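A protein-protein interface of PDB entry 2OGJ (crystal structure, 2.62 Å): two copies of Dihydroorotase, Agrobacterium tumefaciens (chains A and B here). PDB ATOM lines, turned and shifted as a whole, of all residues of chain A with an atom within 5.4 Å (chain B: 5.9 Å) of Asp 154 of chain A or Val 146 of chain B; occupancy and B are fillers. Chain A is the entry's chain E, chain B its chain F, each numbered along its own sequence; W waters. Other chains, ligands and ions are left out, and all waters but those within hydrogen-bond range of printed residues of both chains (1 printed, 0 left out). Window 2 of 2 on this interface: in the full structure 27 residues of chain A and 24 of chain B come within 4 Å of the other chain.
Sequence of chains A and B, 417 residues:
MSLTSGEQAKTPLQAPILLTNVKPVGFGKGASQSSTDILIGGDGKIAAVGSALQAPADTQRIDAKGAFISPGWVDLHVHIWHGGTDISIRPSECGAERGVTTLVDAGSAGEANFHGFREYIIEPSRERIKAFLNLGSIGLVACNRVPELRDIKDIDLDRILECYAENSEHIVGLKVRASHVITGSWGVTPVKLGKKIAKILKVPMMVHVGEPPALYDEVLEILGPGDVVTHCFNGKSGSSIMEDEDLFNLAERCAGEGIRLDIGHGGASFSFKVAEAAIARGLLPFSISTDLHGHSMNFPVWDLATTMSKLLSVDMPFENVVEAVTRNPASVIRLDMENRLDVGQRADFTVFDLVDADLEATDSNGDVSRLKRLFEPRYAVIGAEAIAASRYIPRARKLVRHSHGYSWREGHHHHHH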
ATOM      1  N   LEU A 135      -7.575 -25.038   9.243  1.00  0.00           N
ATOM      2  CA  LEU A 135      -8.619 -25.013  10.256  1.00  0.00           C
ATOM      3  C   LEU A 135      -7.942 -24.619  11.590  1.00  0.00           C
ATOM      4  O   LEU A 135      -8.569 -23.984  12.445  1.00  0.00           O
ATOM      5  CB  LEU A 135      -9.257 -26.397  10.365  1.00  0.00           C
ATOM      6  CG  LEU A 135     -10.740 -26.521  10.723  1.00  0.00           C
ATOM      7  CD1 LEU A 135     -10.981 -27.960  11.153  1.00  0.00           C
ATOM      8  CD2 LEU A 135     -11.136 -25.576  11.834  1.00  0.00           C
ATOM      9  N   GLY A 136      -6.656 -24.981  11.730  1.00  0.00           N
ATOM     10  CA  GLY A 136      -5.869 -24.678  12.924  1.00  0.00           C
ATOM     11  C   GLY A 136      -5.206 -23.303  12.898  1.00  0.00           C
ATOM     12  O   GLY A 136      -4.520 -22.944  11.943  1.00  0.00           O
ATOM     13  N   SER A 137      -5.394 -22.545  13.972  1.00  0.00           N
ATOM     14  CA  SER A 137      -4.864 -21.188  14.077  1.00  0.00           C
ATOM     15  C   SER A 137      -3.383 -20.914  13.756  1.00  0.00           C
ATOM     16  O   SER A 137      -3.077 -19.952  13.044  1.00  0.00           O
ATOM     17  CB  SER A 137      -5.184 -20.626  15.466  1.00  0.00           C
ATOM     18  OG  SER A 137      -6.562 -20.322  15.573  1.00  0.00           O
ATOM     19  N   ILE A 138      -2.471 -21.724  14.295  1.00  0.00           N
ATOM     20  CA  ILE A 138      -1.040 -21.526  14.050  1.00  0.00           C
ATOM     21  C   ILE A 138      -0.535 -22.139  12.738  1.00  0.00           C
ATOM     22  O   ILE A 138       0.625 -21.938  12.369  1.00  0.00           O
ATOM     23  CB  ILE A 138      -0.175 -22.112  15.196  1.00  0.00           C
ATOM     24  CG1 ILE A 138      -0.094 -23.636  15.068  1.00  0.00           C
ATOM     25  CG2 ILE A 138      -0.753 -21.713  16.558  1.00  0.00           C
ATOM     26  CD1 ILE A 138       0.726 -24.294  16.163  1.00  0.00           C
ATOM     27  N   PRO A 147       1.736 -29.661  16.303  1.00  0.00           N
ATOM     28  CA  PRO A 147       0.447 -29.788  15.607  1.00  0.00           C
ATOM     29  C   PRO A 147      -0.501 -28.586  15.707  1.00  0.00           C
ATOM     30  O   PRO A 147      -0.715 -28.034  16.779  1.00  0.00           O
ATOM     31  CB  PRO A 147      -0.154 -31.038  16.246  1.00  0.00           C
ATOM     32  CG  PRO A 147       1.062 -31.904  16.469  1.00  0.00           C
ATOM     33  CD  PRO A 147       2.075 -30.914  17.017  1.00  0.00           C
ATOM     34  N   GLU A 148      -1.091 -28.202  14.581  1.00  0.00           N
ATOM     35  CA  GLU A 148      -2.027 -27.083  14.550  1.00  0.00           C
ATOM     36  C   GLU A 148      -3.460 -27.528  14.888  1.00  0.00           C
ATOM     37  O   GLU A 148      -4.362 -26.694  14.976  1.00  0.00           O
ATOM     38  CB  GLU A 148      -2.002 -26.398  13.172  1.00  0.00           C
ATOM     39  CG  GLU A 148      -2.653 -27.169  12.036  1.00  0.00           C
ATOM     40  CD  GLU A 148      -1.785 -28.292  11.469  1.00  0.00           C
ATOM     41  OE1 GLU A 148      -2.102 -28.802  10.365  1.00  0.00           O
ATOM     42  OE2 GLU A 148      -0.794 -28.675  12.120  1.00  0.00           O
ATOM     43  N   LEU A 149      -3.661 -28.835  15.082  1.00  0.00           N
ATOM     44  CA  LEU A 149      -4.985 -29.382  15.410  1.00  0.00           C
ATOM     45  C   LEU A 149      -4.933 -30.426  16.538  1.00  0.00           C
ATOM     46  O   LEU A 149      -5.189 -31.610  16.308  1.00  0.00           O
ATOM     47  CB  LEU A 149      -5.605 -30.011  14.154  1.00  0.00           C
ATOM     48  CG  LEU A 149      -6.952 -29.488  13.621  1.00  0.00           C
ATOM     49  CD1 LEU A 149      -6.996 -27.959  13.617  1.00  0.00           C
ATOM     50  CD2 LEU A 149      -7.169 -30.059  12.219  1.00  0.00           C
ATOM     51  N   ARG A 150      -4.618 -29.981  17.753  1.00  0.00           N
ATOM     52  CA  ARG A 150      -4.513 -30.880  18.904  1.00  0.00           C
ATOM     53  C   ARG A 150      -5.792 -30.973  19.725  1.00  0.00           C
ATOM     54  O   ARG A 150      -6.158 -32.049  20.186  1.00  0.00           O
ATOM     55  CB  ARG A 150      -3.358 -30.440  19.812  1.00  0.00           C
ATOM     56  CG  ARG A 150      -1.976 -30.673  19.215  1.00  0.00           C
ATOM     57  CD  ARG A 150      -0.849 -30.202  20.140  1.00  0.00           C
ATOM     58  NE  ARG A 150      -0.783 -28.745  20.266  1.00  0.00           N
ATOM     59  CZ  ARG A 150       0.095 -28.093  21.030  1.00  0.00           C
ATOM     60  NH1 ARG A 150       0.988 -28.778  21.748  1.00  0.00           N
ATOM     61  NH2 ARG A 150       0.084 -26.759  21.069  1.00  0.00           N
ATOM     62  N   ASP A 151      -6.464 -29.844  19.913  1.00  0.00           N
ATOM     63  CA  ASP A 151      -7.708 -29.787  20.677  1.00  0.00           C
ATOM     64  C   ASP A 151      -8.569 -28.669  20.099  1.00  0.00           C
ATOM     65  O   ASP A 151      -8.162 -28.031  19.138  1.00  0.00           O
ATOM     66  CB  ASP A 151      -7.400 -29.509  22.150  1.00  0.00           C
ATOM     67  CG  ASP A 151      -6.397 -28.394  22.335  1.00  0.00           C
ATOM     68  OD1 ASP A 151      -6.711 -27.236  21.983  1.00  0.00           O
ATOM     69  OD2 ASP A 151      -5.288 -28.685  22.829  1.00  0.00           O
ATOM     70  N   ILE A 152      -9.752 -28.410  20.650  1.00  0.00           N
ATOM     71  CA  ILE A 152     -10.542 -27.338  20.066  1.00  0.00           C
ATOM     72  C   ILE A 152      -9.956 -25.978  20.326  1.00  0.00           C
ATOM     73  O   ILE A 152     -10.312 -25.029  19.640  1.00  0.00           O
ATOM     74  CB  ILE A 152     -12.041 -27.328  20.514  1.00  0.00           C
ATOM     75  CG1 ILE A 152     -12.205 -27.883  21.930  1.00  0.00           C
ATOM     76  CG2 ILE A 152     -12.877 -28.058  19.479  1.00  0.00           C
ATOM     77  CD1 ILE A 152     -11.954 -26.883  23.029  1.00  0.00           C
ATOM     78  N   LYS A 153      -9.059 -25.861  21.300  1.00  0.00           N
ATOM     79  CA  LYS A 153      -8.482 -24.551  21.560  1.00  0.00           C
ATOM     80  C   LYS A 153      -7.717 -24.061  20.318  1.00  0.00           C
ATOM     81  O   LYS A 153      -7.371 -22.872  20.214  1.00  0.00           O
ATOM     82  CB  LYS A 153      -7.557 -24.578  22.790  1.00  0.00           C
ATOM     83  CG  LYS A 153      -8.282 -24.846  24.120  1.00  0.00           C
ATOM     84  CD  LYS A 153      -7.624 -24.170  25.347  1.00  0.00           C
ATOM     85  CE  LYS A 153      -6.244 -24.759  25.734  1.00  0.00           C
ATOM     86  NZ  LYS A 153      -5.044 -24.083  25.106  1.00  0.00           N
ATOM     87  N   ASP A 154      -7.479 -24.971  19.367  1.00  0.00           N
ATOM     88  CA  ASP A 154      -6.769 -24.626  18.133  1.00  0.00           C
ATOM     89  C   ASP A 154      -7.700 -24.031  17.063  1.00  0.00           C
ATOM     90  O   ASP A 154      -7.327 -23.108  16.348  1.00  0.00           O
ATOM     91  CB  ASP A 154      -6.040 -25.849  17.572  1.00  0.00           C
ATOM     92  CG  ASP A 154      -4.817 -26.246  18.405  1.00  0.00           C
ATOM     93  OD1 ASP A 154      -4.164 -25.341  18.971  1.00  0.00           O
ATOM     94  OD2 ASP A 154      -4.499 -27.459  18.476  1.00  0.00           O
ATOM     95  N   ILE A 155      -8.911 -24.556  16.961  1.00  0.00           N
ATOM     96  CA  ILE A 155      -9.895 -24.060  16.004  1.00  0.00           C
ATOM     97  C   ILE A 155     -10.684 -22.881  16.579  1.00  0.00           C
ATOM     98  O   ILE A 155     -11.295 -22.999  17.634  1.00  0.00           O
ATOM     99  CB  ILE A 155     -10.912 -25.144  15.657  1.00  0.00           C
ATOM    100  CG1 ILE A 155     -10.188 -26.358  15.079  1.00  0.00           C
ATOM    101  CG2 ILE A 155     -11.982 -24.573  14.725  1.00  0.00           C
ATOM    102  CD1 ILE A 155     -11.075 -27.551  14.908  1.00  0.00           C
ATOM    103  N   ASP A 156     -10.683 -21.747  15.889  1.00  0.00           N
ATOM    104  CA  ASP A 156     -11.424 -20.585  16.359  1.00  0.00           C
ATOM    105  C   ASP A 156     -12.341 -20.081  15.248  1.00  0.00           C
ATOM    106  O   ASP A 156     -11.939 -19.280  14.409  1.00  0.00           O
ATOM    107  CB  ASP A 156     -10.462 -19.485  16.817  1.00  0.00           C
ATOM    108  CG  ASP A 156     -11.187 -18.273  17.368  1.00  0.00           C
ATOM    109  OD1 ASP A 156     -10.607 -17.542  18.207  1.00  0.00           O
ATOM    110  OD2 ASP A 156     -12.341 -18.046  16.950  1.00  0.00           O
ATOM    111  N   ILE B 138       6.866 -22.148  18.351  1.00  0.00           N
ATOM    112  CA  ILE B 138       5.914 -21.338  17.601  1.00  0.00           C
ATOM    113  C   ILE B 138       5.926 -19.867  17.997  1.00  0.00           C
ATOM    114  O   ILE B 138       5.311 -19.032  17.339  1.00  0.00           O
ATOM    115  CB  ILE B 138       4.480 -21.885  17.738  1.00  0.00           C
ATOM    116  CG1 ILE B 138       3.977 -21.719  19.177  1.00  0.00           C
ATOM    117  CG2 ILE B 138       4.455 -23.352  17.336  1.00  0.00           C
ATOM    118  CD1 ILE B 138       2.578 -22.312  19.423  1.00  0.00           C
ATOM    119  N   GLY B 139       6.649 -19.533  19.055  1.00  0.00           N
ATOM    120  CA  GLY B 139       6.679 -18.145  19.462  1.00  0.00           C
ATOM    121  C   GLY B 139       5.271 -17.648  19.698  1.00  0.00           C
ATOM    122  O   GLY B 139       4.418 -18.383  20.175  1.00  0.00           O
ATOM    123  N   ALA B 142      -0.050 -17.082  17.630  1.00  0.00           N
ATOM    124  CA  ALA B 142      -1.403 -16.774  18.089  1.00  0.00           C
ATOM    125  C   ALA B 142      -1.299 -16.502  19.587  1.00  0.00           C
ATOM    126  O   ALA B 142      -1.755 -17.292  20.415  1.00  0.00           O
ATOM    127  CB  ALA B 142      -2.334 -17.962  17.825  1.00  0.00           C
ATOM    128  N   CYS B 143      -0.707 -15.361  19.916  1.00  0.00           N
ATOM    129  CA  CYS B 143      -0.444 -14.983  21.299  1.00  0.00           C
ATOM    130  C   CYS B 143      -1.535 -15.207  22.335  1.00  0.00           C
ATOM    131  O   CYS B 143      -2.645 -14.671  22.241  1.00  0.00           O
ATOM    132  CB  CYS B 143       0.031 -13.530  21.361  1.00  0.00           C
ATOM    133  SG  CYS B 143       0.699 -13.058  22.967  1.00  0.00           S
ATOM    134  N   ASN B 144      -1.177 -16.003  23.340  1.00  0.00           N
ATOM    135  CA  ASN B 144      -2.067 -16.360  24.439  1.00  0.00           C
ATOM    136  C   ASN B 144      -3.164 -17.357  24.056  1.00  0.00           C
ATOM    137  O   ASN B 144      -3.504 -18.236  24.842  1.00  0.00           O
ATOM    138  CB  ASN B 144      -2.669 -15.094  25.055  1.00  0.00           C
ATOM    139  CG  ASN B 144      -1.632 -14.280  25.812  1.00  0.00           C
ATOM    140  OD1 ASN B 144      -0.491 -14.705  25.949  1.00  0.00           O
ATOM    141  ND2 ASN B 144      -2.026 -13.116  26.311  1.00  0.00           N
ATOM    142  N   ARG B 145      -3.707 -17.232  22.851  1.00  0.00           N
ATOM    143  CA  ARG B 145      -4.747 -18.140  22.378  1.00  0.00           C
ATOM    144  C   ARG B 145      -4.170 -19.555  22.206  1.00  0.00           C
ATOM    145  O   ARG B 145      -4.853 -20.556  22.425  1.00  0.00           O
ATOM    146  CB  ARG B 145      -5.297 -17.618  21.056  1.00  0.00           C
ATOM    147  CG  ARG B 145      -5.524 -16.107  21.085  1.00  0.00           C
ATOM    148  CD  ARG B 145      -6.393 -15.618  19.937  1.00  0.00           C
ATOM    149  NE  ARG B 145      -5.639 -15.337  18.719  1.00  0.00           N
ATOM    150  CZ  ARG B 145      -5.872 -15.924  17.546  1.00  0.00           C
ATOM    151  NH1 ARG B 145      -6.833 -16.830  17.439  1.00  0.00           N
ATOM    152  NH2 ARG B 145      -5.160 -15.593  16.477  1.00  0.00           N
ATOM    153  N   VAL B 146      -2.899 -19.619  21.813  1.00  0.00           N
ATOM    154  CA  VAL B 146      -2.209 -20.889  21.620  1.00  0.00           C
ATOM    155  C   VAL B 146      -0.797 -20.811  22.186  1.00  0.00           C
ATOM    156  O   VAL B 146       0.165 -20.617  21.455  1.00  0.00           O
ATOM    157  CB  VAL B 146      -2.151 -21.275  20.132  1.00  0.00           C
ATOM    158  CG1 VAL B 146      -1.326 -22.533  19.943  1.00  0.00           C
ATOM    159  CG2 VAL B 146      -3.549 -21.528  19.635  1.00  0.00           C
ATOM    160  N   PRO B 147      -0.668 -20.957  23.515  1.00  0.00           N
ATOM    161  CA  PRO B 147       0.579 -20.922  24.295  1.00  0.00           C
ATOM    162  C   PRO B 147       1.812 -21.591  23.656  1.00  0.00           C
ATOM    163  O   PRO B 147       1.739 -22.733  23.178  1.00  0.00           O
ATOM    164  CB  PRO B 147       0.169 -21.605  25.598  1.00  0.00           C
ATOM    165  CG  PRO B 147      -1.230 -21.126  25.777  1.00  0.00           C
ATOM    166  CD  PRO B 147      -1.810 -21.302  24.387  1.00  0.00           C
ATOM    167  N   GLU B 148       2.945 -20.879  23.668  1.00  0.00           N
ATOM    168  CA  GLU B 148       4.198 -21.401  23.094  1.00  0.00           C
ATOM    169  C   GLU B 148       4.928 -22.409  23.988  1.00  0.00           C
ATOM    170  O   GLU B 148       5.725 -23.190  23.498  1.00  0.00           O
ATOM    171  CB  GLU B 148       5.161 -20.261  22.742  1.00  0.00           C
ATOM    172  CG  GLU B 148       5.633 -19.444  23.932  1.00  0.00           C
ATOM    173  CD  GLU B 148       4.671 -18.341  24.326  1.00  0.00           C
ATOM    174  OE1 GLU B 148       5.086 -17.430  25.070  1.00  0.00           O
ATOM    175  OE2 GLU B 148       3.502 -18.373  23.897  1.00  0.00           O
ATOM    176  N   ARG B 150       3.525 -24.971  26.072  1.00  0.00           N
ATOM    177  CA  ARG B 150       2.497 -25.869  26.591  1.00  0.00           C
ATOM    178  C   ARG B 150       3.115 -27.020  27.363  1.00  0.00           C
ATOM    179  O   ARG B 150       2.738 -27.302  28.499  1.00  0.00           O
ATOM    180  CB  ARG B 150       1.636 -26.436  25.455  1.00  0.00           C
ATOM    181  CG  ARG B 150       0.706 -25.431  24.787  1.00  0.00           C
ATOM    182  CD  ARG B 150      -0.667 -26.057  24.588  1.00  0.00           C
ATOM    183  NE  ARG B 150      -1.235 -25.788  23.270  1.00  0.00           N
ATOM    184  CZ  ARG B 150      -2.417 -26.251  22.870  1.00  0.00           C
ATOM    185  NH1 ARG B 150      -3.147 -26.998  23.691  1.00  0.00           N
ATOM    186  NH2 ARG B 150      -2.878 -25.969  21.657  1.00  0.00           N
HETATM  187  O   HOH W   1       1.876 -24.698  21.563  1.00  0.00           O
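Among the printed residues, merely in contact across the chains: Ser 137 of chain A with Arg 145 of chain B, Ile 138 of chain A with Val 146 of chain B, Lys 153 of chain A with Arg 150 of chain B and Asp 154 of chain A with Val 146 of chain B.
Water W1 bridges the backbone carbonyl oxygen (O) of Pro 147 of chain B (2.5 Å) and the guanidinium group (NH2) of Arg 150 of chain A (2.8 Å).
OD2 of Asp 151 of chain A is in salt-bridge range of NH1 of Arg 150 of chain B (2.9 Å).
NE of Arg 150 of chain B sits close to NH2 of Arg 150 of chain A.
The side-chain carboxylate (OD1) of Asp 156 of chain A is in salt-bridge range of the guanidinium group (NH1) of Arg 145 of chain B (3.9 Å).
OD1 of Asp 154 of chain A is in salt-bridge range of NH2 of Arg 150 of chain B, at 3.0 Å.
Arg 150 of chain A touches its own counterpart, Arg 150 of chain B.
Of the 10 printed residues of chain B, 3 touch a printed residue of chain A.
Hydrophobic or aromatic side chains of chain B within 4 Å of the printed part of chain A: Val 146.
Among the printed residues, 8 pairs touch across the chains.
N of Arg 150 of chain A sits at hydrogen-bond distance from OD2 of Asp 154 of chain A (2.6 Å).
OG of Ser 137 of chain A sits at hydrogen-bond distance from O of Asp 154 of chain A.
OD1 of Asp 151 of chain A is in hydrogen-bond range of N of Lys 153 of chain A, at 2.8 Å.
The side-chain carboxylate of Asp 154 of chain A sits at hydrogen-bond distance from the backbone NH of Asp 151 of chain A (3.4 Å).
Printed residues of chain B within 4 Å of Ser 137 of chain A: Arg 145.
Of the printed residues of chain B, Arg 150 of chain A touches Arg 150 (2.7 Å).
Of the printed residues of chain B, Asp 151 of chain A touches Arg 150.
Of the printed residues of chain B, Lys 153 of chain A touches Arg 150 (3.8 Å).
Of chain B, only Val 146 and Arg 150 come within 4 Å of Asp 154 of chain A.
Printed residues of chain A within 4 Å of Arg 145 of chain B: Ser 137 and Asp 156.
Val 146 of chain B touches just these residues of chain A: Ile 138 and Asp 154.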
